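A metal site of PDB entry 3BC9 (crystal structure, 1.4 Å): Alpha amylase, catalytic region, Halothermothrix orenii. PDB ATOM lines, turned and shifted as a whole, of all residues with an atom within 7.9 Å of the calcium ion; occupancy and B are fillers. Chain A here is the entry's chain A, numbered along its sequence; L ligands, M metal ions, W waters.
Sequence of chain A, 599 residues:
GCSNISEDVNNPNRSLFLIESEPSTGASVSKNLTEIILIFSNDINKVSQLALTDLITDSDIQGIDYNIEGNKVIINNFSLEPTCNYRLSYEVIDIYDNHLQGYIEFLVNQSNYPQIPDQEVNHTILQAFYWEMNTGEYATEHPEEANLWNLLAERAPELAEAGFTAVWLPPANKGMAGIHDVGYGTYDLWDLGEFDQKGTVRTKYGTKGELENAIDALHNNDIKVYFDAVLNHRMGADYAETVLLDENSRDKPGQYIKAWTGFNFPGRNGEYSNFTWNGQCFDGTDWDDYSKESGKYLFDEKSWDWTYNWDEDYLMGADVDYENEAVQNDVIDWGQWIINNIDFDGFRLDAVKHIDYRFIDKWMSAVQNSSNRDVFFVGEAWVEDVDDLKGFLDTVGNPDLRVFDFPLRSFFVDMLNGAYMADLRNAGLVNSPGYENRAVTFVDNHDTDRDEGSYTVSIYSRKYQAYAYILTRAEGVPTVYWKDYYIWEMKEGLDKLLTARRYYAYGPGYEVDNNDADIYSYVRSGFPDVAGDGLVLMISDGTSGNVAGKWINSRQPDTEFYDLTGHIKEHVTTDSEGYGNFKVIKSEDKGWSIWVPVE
Water W1 bridges the backbone NH (N) of Ser 303 (3.1 Å) and the side-chain carboxylate (OD2) of Asp 321 (3.2 Å).
Within 4 Å of the calcium ion: Asp 283, Ser 303, Asp 305, Asp 321 and Glu 323.
Along chain A the residues within 4 Å of the calcium ion span positions 283 to 323.
The nearest printed residue that does not touch the calcium ion is Trp 304 (4.2 Å).
N of Asp 321 lies within hydrogen-bond range of O of Cys 281, at 2.9 Å.
OD2 of Asp 313 is in hydrogen-bond range of N of Asp 305, 2.8 Å away.
OD2 of Asp 321 is in salt-bridge range of NZ of Lys 302 (2.7 Å).
NH2 of Arg 358 lies within salt-bridge range of OE2 of Glu 323 (3.0 Å).
The side-chain carboxylate of Asp 305 is in hydrogen-bond range of the backbone NH of Tyr 322, at 3.0 Å.
The backbone NH (N) of Asp 283 lies within hydrogen-bond range of the backbone carbonyl oxygen (O) of Asp 319, 2.8 Å away.
O of Trp 304 sits at hydrogen-bond distance from O2 of the ligand, 2.8 Å away.
The calcium ion is bound by the side-chain carboxylate (OD1) of Asp 305 (2.3 Å), the side-chain carboxylate (OE1) of Glu 323 (2.3 Å), the backbone carbonyl oxygen (O) of Ser 303 (2.4 Å), the side-chain carboxylate (OD1) of Asp 321 (2.4 Å), water W1 (2.5 Å), the side-chain carboxylate (OD2) of Asp 283 (2.5 Å) and the side-chain carboxylate (OD1) of Asp 283 (2.6 Å).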
ATOM      1  N   CYS A 281     -25.613  17.994 -11.214  1.00  0.00           N
ATOM      2  CA  CYS A 281     -26.965  18.339 -10.802  1.00  0.00           C
ATOM      3  C   CYS A 281     -27.850  17.075 -10.588  1.00  0.00           C
ATOM      4  O   CYS A 281     -29.025  17.208 -10.239  1.00  0.00           O
ATOM      5  CB  CYS A 281     -27.612  19.141 -11.912  1.00  0.00           C
ATOM      6  SG  CYS A 281     -26.827  20.730 -12.149  1.00  0.00           S
ATOM      7  N   PHE A 282     -27.297  15.906 -10.899  1.00  0.00           N
ATOM      8  CA  PHE A 282     -28.024  14.620 -10.935  1.00  0.00           C
ATOM      9  C   PHE A 282     -27.374  13.625 -10.023  1.00  0.00           C
ATOM     10  O   PHE A 282     -26.150  13.673  -9.824  1.00  0.00           O
ATOM     11  CB  PHE A 282     -28.127  14.086 -12.357  1.00  0.00           C
ATOM     12  CG  PHE A 282     -28.860  14.968 -13.302  1.00  0.00           C
ATOM     13  CD1 PHE A 282     -28.171  15.735 -14.223  1.00  0.00           C
ATOM     14  CD2 PHE A 282     -30.228  15.116 -13.285  1.00  0.00           C
ATOM     15  CE1 PHE A 282     -28.806  16.555 -15.109  1.00  0.00           C
ATOM     16  CE2 PHE A 282     -30.891  15.968 -14.114  1.00  0.00           C
ATOM     17  CZ  PHE A 282     -30.177  16.695 -15.103  1.00  0.00           C
ATOM     18  N   ASP A 283     -28.176  12.720  -9.415  1.00  0.00           N
ATOM     19  CA  ASP A 283     -27.628  11.633  -8.671  1.00  0.00           C
ATOM     20  C   ASP A 283     -27.247  10.439  -9.502  1.00  0.00           C
ATOM     21  O   ASP A 283     -26.368   9.666  -9.134  1.00  0.00           O
ATOM     22  CB  ASP A 283     -28.592  11.131  -7.592  1.00  0.00           C
ATOM     23  CG  ASP A 283     -28.669  12.081  -6.393  1.00  0.00           C
ATOM     24  OD1 ASP A 283     -27.526  12.615  -6.092  1.00  0.00           O
ATOM     25  OD2 ASP A 283     -29.752  12.363  -5.734  1.00  0.00           O
ATOM     26  N   GLY A 284     -27.956  10.242 -10.601  1.00  0.00           N
ATOM     27  CA  GLY A 284     -27.685   9.081 -11.418  1.00  0.00           C
ATOM     28  C   GLY A 284     -28.620   9.002 -12.616  1.00  0.00           C
ATOM     29  O   GLY A 284     -29.346   9.918 -12.909  1.00  0.00           O
ATOM     30  N   LEU A 298     -25.350   5.142 -10.019  1.00  0.00           N
ATOM     31  CA  LEU A 298     -25.165   6.226  -9.097  1.00  0.00           C
ATOM     32  C   LEU A 298     -23.833   6.937  -9.395  1.00  0.00           C
ATOM     33  O   LEU A 298     -22.813   6.254  -9.402  1.00  0.00           O
ATOM     34  CB  LEU A 298     -25.115   5.654  -7.672  1.00  0.00           C
ATOM     35  CG  LEU A 298     -24.975   6.650  -6.489  1.00  0.00           C
ATOM     36  CD1 LEU A 298     -26.058   7.661  -6.368  1.00  0.00           C
ATOM     37  CD2 LEU A 298     -24.660   5.919  -5.214  1.00  0.00           C
ATOM     38  N   GLU A 301     -19.561  10.207  -5.793  1.00  0.00           N
ATOM     39  CA  GLU A 301     -19.771  11.113  -4.700  1.00  0.00           C
ATOM     40  C   GLU A 301     -21.213  11.562  -4.497  1.00  0.00           C
ATOM     41  O   GLU A 301     -21.504  12.336  -3.572  1.00  0.00           O
ATOM     42  CB  GLU A 301     -18.875  12.348  -4.781  1.00  0.00           C
ATOM     43  CG  GLU A 301     -17.403  12.061  -4.677  1.00  0.00           C
ATOM     44  CD  GLU A 301     -16.601  13.340  -4.786  1.00  0.00           C
ATOM     45  OE1 GLU A 301     -16.344  13.968  -3.745  1.00  0.00           O
ATOM     46  OE2 GLU A 301     -16.284  13.768  -5.934  1.00  0.00           O
ATOM     47  N   LYS A 302     -22.128  11.016  -5.271  1.00  0.00           N
ATOM     48  CA  LYS A 302     -23.542  11.328  -5.058  1.00  0.00           C
ATOM     49  C   LYS A 302     -24.141  10.296  -4.114  1.00  0.00           C
ATOM     50  O   LYS A 302     -23.618   9.213  -3.926  1.00  0.00           O
ATOM     51  CB  LYS A 302     -24.285  11.332  -6.377  1.00  0.00           C
ATOM     52  CG  LYS A 302     -23.882  12.433  -7.295  1.00  0.00           C
ATOM     53  CD  LYS A 302     -24.141  13.805  -6.746  1.00  0.00           C
ATOM     54  CE  LYS A 302     -23.897  14.891  -7.804  1.00  0.00           C
ATOM     55  NZ  LYS A 302     -24.198  16.147  -7.102  1.00  0.00           N
ATOM     56  N   SER A 303     -25.307  10.640  -3.613  1.00  0.00           N
ATOM     57  CA  SER A 303     -26.062   9.704  -2.806  1.00  0.00           C
ATOM     58  C   SER A 303     -27.538   9.882  -3.138  1.00  0.00           C
ATOM     59  O   SER A 303     -27.970  11.003  -3.336  1.00  0.00           O
ATOM     60  CB  SER A 303     -25.839   9.937  -1.321  1.00  0.00           C
ATOM     61  OG  SER A 303     -25.939  11.257  -0.989  1.00  0.00           O
ATOM     62  N   TRP A 304     -28.300   8.818  -3.131  1.00  0.00           N
ATOM     63  CA  TRP A 304     -29.727   8.962  -3.356  1.00  0.00           C
ATOM     64  C   TRP A 304     -30.293   9.800  -2.211  1.00  0.00           C
ATOM     65  O   TRP A 304     -29.914   9.692  -1.033  1.00  0.00           O
ATOM     66  CB  TRP A 304     -30.377   7.610  -3.425  1.00  0.00           C
ATOM     67  CG  TRP A 304     -29.868   6.703  -4.497  1.00  0.00           C
ATOM     68  CD1 TRP A 304     -29.349   5.484  -4.328  1.00  0.00           C
ATOM     69  CD2 TRP A 304     -29.888   6.945  -5.922  1.00  0.00           C
ATOM     70  NE1 TRP A 304     -28.991   4.958  -5.539  1.00  0.00           N
ATOM     71  CE2 TRP A 304     -29.342   5.814  -6.542  1.00  0.00           C
ATOM     72  CE3 TRP A 304     -30.305   8.001  -6.715  1.00  0.00           C
ATOM     73  CZ2 TRP A 304     -29.141   5.752  -7.921  1.00  0.00           C
ATOM     74  CZ3 TRP A 304     -30.118   7.943  -8.055  1.00  0.00           C
ATOM     75  CH2 TRP A 304     -29.548   6.809  -8.661  1.00  0.00           C
ATOM     76  N   ASP A 305     -31.258  10.629  -2.572  1.00  0.00           N
ATOM     77  CA  ASP A 305     -31.872  11.568  -1.683  1.00  0.00           C
ATOM     78  C   ASP A 305     -32.784  10.809  -0.697  1.00  0.00           C
ATOM     79  O   ASP A 305     -33.160   9.668  -0.894  1.00  0.00           O
ATOM     80  CB  ASP A 305     -32.609  12.622  -2.460  1.00  0.00           C
ATOM     81  CG  ASP A 305     -31.731  13.465  -3.384  1.00  0.00           C
ATOM     82  OD1 ASP A 305     -30.570  13.648  -2.978  1.00  0.00           O
ATOM     83  OD2 ASP A 305     -32.348  13.961  -4.374  1.00  0.00           O
ATOM     84  N   TRP A 306     -33.203  11.501   0.348  1.00  0.00           N
ATOM     85  CA  TRP A 306     -34.011  10.876   1.420  1.00  0.00           C
ATOM     86  C   TRP A 306     -35.422  10.764   0.905  1.00  0.00           C
ATOM     87  O   TRP A 306     -36.090  11.761   0.642  1.00  0.00           O
ATOM     88  CB  TRP A 306     -33.944  11.700   2.699  1.00  0.00           C
ATOM     89  CG  TRP A 306     -32.671  11.761   3.331  1.00  0.00           C
ATOM     90  CD1 TRP A 306     -31.448  11.468   2.810  1.00  0.00           C
ATOM     91  CD2 TRP A 306     -32.432  12.231   4.646  1.00  0.00           C
ATOM     92  NE1 TRP A 306     -30.450  11.655   3.761  1.00  0.00           N
ATOM     93  CE2 TRP A 306     -31.039  12.175   4.873  1.00  0.00           C
ATOM     94  CE3 TRP A 306     -33.272  12.710   5.647  1.00  0.00           C
ATOM     95  CZ2 TRP A 306     -30.475  12.573   6.092  1.00  0.00           C
ATOM     96  CZ3 TRP A 306     -32.703  13.100   6.870  1.00  0.00           C
ATOM     97  CH2 TRP A 306     -31.335  13.056   7.057  1.00  0.00           C
ATOM     98  N   ASP A 313     -35.527   6.918  -4.414  1.00  0.00           N
ATOM     99  CA  ASP A 313     -35.255   8.146  -5.194  1.00  0.00           C
ATOM    100  C   ASP A 313     -35.217   7.850  -6.718  1.00  0.00           C
ATOM    101  O   ASP A 313     -35.757   8.597  -7.496  1.00  0.00           O
ATOM    102  CB  ASP A 313     -33.902   8.693  -4.784  1.00  0.00           C
ATOM    103  CG  ASP A 313     -33.593  10.094  -5.268  1.00  0.00           C
ATOM    104  OD1 ASP A 313     -34.514  10.812  -5.700  1.00  0.00           O
ATOM    105  OD2 ASP A 313     -32.420  10.519  -5.082  1.00  0.00           O
ATOM    106  N   ASP A 319     -31.828  11.475 -12.687  1.00  0.00           N
ATOM    107  CA  ASP A 319     -32.505  11.756 -11.420  1.00  0.00           C
ATOM    108  C   ASP A 319     -31.934  13.014 -10.813  1.00  0.00           C
ATOM    109  O   ASP A 319     -30.743  13.041 -10.532  1.00  0.00           O
ATOM    110  CB  ASP A 319     -32.321  10.567 -10.501  1.00  0.00           C
ATOM    111  CG  ASP A 319     -33.101  10.752  -9.201  1.00  0.00           C
ATOM    112  OD1 ASP A 319     -34.299  10.529  -9.321  1.00  0.00           O
ATOM    113  OD2 ASP A 319     -32.469  11.059  -8.190  1.00  0.00           O
ATOM    114  N   VAL A 320     -32.790  13.954 -10.502  1.00  0.00           N
ATOM    115  CA  VAL A 320     -32.351  15.235  -9.961  1.00  0.00           C
ATOM    116  C   VAL A 320     -31.766  15.016  -8.592  1.00  0.00           C
ATOM    117  O   VAL A 320     -32.313  14.263  -7.787  1.00  0.00           O
ATOM    118  CB  VAL A 320     -33.426  16.291  -9.945  1.00  0.00           C
ATOM    119  CG1 VAL A 320     -32.965  17.585  -9.385  1.00  0.00           C
ATOM    120  CG2 VAL A 320     -33.932  16.480 -11.416  1.00  0.00           C
ATOM    121  N   ASP A 321     -30.618  15.679  -8.304  1.00  0.00           N
ATOM    122  CA  ASP A 321     -29.990  15.674  -6.999  1.00  0.00           C
ATOM    123  C   ASP A 321     -30.497  16.824  -6.200  1.00  0.00           C
ATOM    124  O   ASP A 321     -29.962  17.939  -6.345  1.00  0.00           O
ATOM    125  CB  ASP A 321     -28.467  15.736  -7.091  1.00  0.00           C
ATOM    126  CG  ASP A 321     -27.796  15.724  -5.820  1.00  0.00           C
ATOM    127  OD1 ASP A 321     -28.435  15.480  -4.761  1.00  0.00           O
ATOM    128  OD2 ASP A 321     -26.553  15.962  -5.763  1.00  0.00           O
ATOM    129  N   TYR A 322     -31.507  16.621  -5.342  1.00  0.00           N
ATOM    130  CA  TYR A 322     -32.074  17.705  -4.566  1.00  0.00           C
ATOM    131  C   TYR A 322     -31.268  18.009  -3.330  1.00  0.00           C
ATOM    132  O   TYR A 322     -31.694  18.868  -2.539  1.00  0.00           O
ATOM    133  CB  TYR A 322     -33.555  17.488  -4.275  1.00  0.00           C
ATOM    134  CG  TYR A 322     -34.371  17.815  -5.520  1.00  0.00           C
ATOM    135  CD1 TYR A 322     -35.055  16.879  -6.227  1.00  0.00           C
ATOM    136  CD2 TYR A 322     -34.393  19.114  -5.986  1.00  0.00           C
ATOM    137  CE1 TYR A 322     -35.762  17.202  -7.377  1.00  0.00           C
ATOM    138  CE2 TYR A 322     -35.128  19.462  -7.112  1.00  0.00           C
ATOM    139  CZ  TYR A 322     -35.771  18.483  -7.842  1.00  0.00           C
ATOM    140  OH  TYR A 322     -36.481  18.824  -8.941  1.00  0.00           O
ATOM    141  N   GLU A 323     -30.119  17.425  -3.144  1.00  0.00           N
ATOM    142  CA  GLU A 323     -29.113  17.886  -2.213  1.00  0.00           C
ATOM    143  C   GLU A 323     -28.210  19.007  -2.773  1.00  0.00           C
ATOM    144  O   GLU A 323     -27.452  19.622  -2.010  1.00  0.00           O
ATOM    145  CB  GLU A 323     -28.310  16.722  -1.673  1.00  0.00           C
ATOM    146  CG  GLU A 323     -29.166  15.794  -0.817  1.00  0.00           C
ATOM    147  CD  GLU A 323     -28.649  14.370  -0.610  1.00  0.00           C
ATOM    148  OE1 GLU A 323     -28.031  13.742  -1.521  1.00  0.00           O
ATOM    149  OE2 GLU A 323     -28.868  13.860   0.567  1.00  0.00           O
ATOM    150  N   ASN A 324     -28.252  19.237  -4.089  1.00  0.00           N
ATOM    151  CA  ASN A 324     -27.526  20.314  -4.731  1.00  0.00           C
ATOM    152  C   ASN A 324     -28.266  21.630  -4.554  1.00  0.00           C
ATOM    153  O   ASN A 324     -29.408  21.781  -5.004  1.00  0.00           O
ATOM    154  CB  ASN A 324     -27.316  19.912  -6.189  1.00  0.00           C
ATOM    155  CG  ASN A 324     -26.608  20.959  -7.008  1.00  0.00           C
ATOM    156  OD1 ASN A 324     -26.945  22.131  -6.946  1.00  0.00           O
ATOM    157  ND2 ASN A 324     -25.701  20.508  -7.863  1.00  0.00           N
ATOM    158  N   ASP A 356     -36.812  13.840  -2.780  1.00  0.00           N
ATOM    159  CA  ASP A 356     -36.361  14.138  -1.439  1.00  0.00           C
ATOM    160  C   ASP A 356     -37.467  14.809  -0.652  1.00  0.00           C
ATOM    161  O   ASP A 356     -37.896  15.896  -0.991  1.00  0.00           O
ATOM    162  CB  ASP A 356     -35.174  15.097  -1.480  1.00  0.00           C
ATOM    163  CG  ASP A 356     -34.434  15.094  -0.198  1.00  0.00           C
ATOM    164  OD1 ASP A 356     -34.990  15.614   0.756  1.00  0.00           O
ATOM    165  OD2 ASP A 356     -33.414  14.412   0.066  1.00  0.00           O
ATOM    166  N   ARG A 358     -37.360  16.260   2.233  1.00  0.00           N
ATOM    167  CA  ARG A 358     -36.892  17.509   2.717  1.00  0.00           C
ATOM    168  C   ARG A 358     -37.068  18.636   1.715  1.00  0.00           C
ATOM    169  O   ARG A 358     -37.508  19.781   2.023  1.00  0.00           O
ATOM    170  CB  ARG A 358     -35.452  17.422   3.144  1.00  0.00           C
ATOM    171  CG  ARG A 358     -35.164  16.343   4.216  1.00  0.00           C
ATOM    172  CD  ARG A 358     -33.642  16.090   4.325  1.00  0.00           C
ATOM    173  NE  ARG A 358     -33.104  15.580   3.089  1.00  0.00           N
ATOM    174  CZ  ARG A 358     -31.834  15.257   2.895  1.00  0.00           C
ATOM    175  NH1 ARG A 358     -30.979  15.426   3.893  1.00  0.00           N
ATOM    176  NH2 ARG A 358     -31.421  14.799   1.717  1.00  0.00           N
HETATM  177  C1  LIG L   1     -31.372   5.913  -0.034  1.00  0.00           C
HETATM  178  C2  LIG L   1     -30.689   7.146   0.571  1.00  0.00           C
HETATM  179  C3  LIG L   1     -30.798   7.121   2.061  1.00  0.00           C
HETATM  180  C4  LIG L   1     -32.230   7.437   2.192  1.00  0.00           C
HETATM  181  C5  LIG L   1     -33.048   6.266   1.649  1.00  0.00           C
HETATM  182  C6  LIG L   1     -34.352   6.944   1.551  1.00  0.00           C
HETATM  183  O1  LIG L   1     -30.709   4.728   0.320  1.00  0.00           O
HETATM  184  O2  LIG L   1     -29.350   7.281   0.228  1.00  0.00           O
HETATM  185  O3  LIG L   1     -30.146   8.214   2.667  1.00  0.00           O
HETATM  186  O4  LIG L   1     -32.586   7.726   3.512  1.00  0.00           O
HETATM  187  O5  LIG L   1     -32.738   5.798   0.347  1.00  0.00           O
HETATM  188  O6  LIG L   1     -34.661   7.410   2.807  1.00  0.00           O
HETATM  189 CA    CA M   1     -28.466  13.282  -3.780  1.00  0.00          CA
HETATM  190  O   HOH W   1     -26.017  13.642  -3.663  1.00  0.00           O
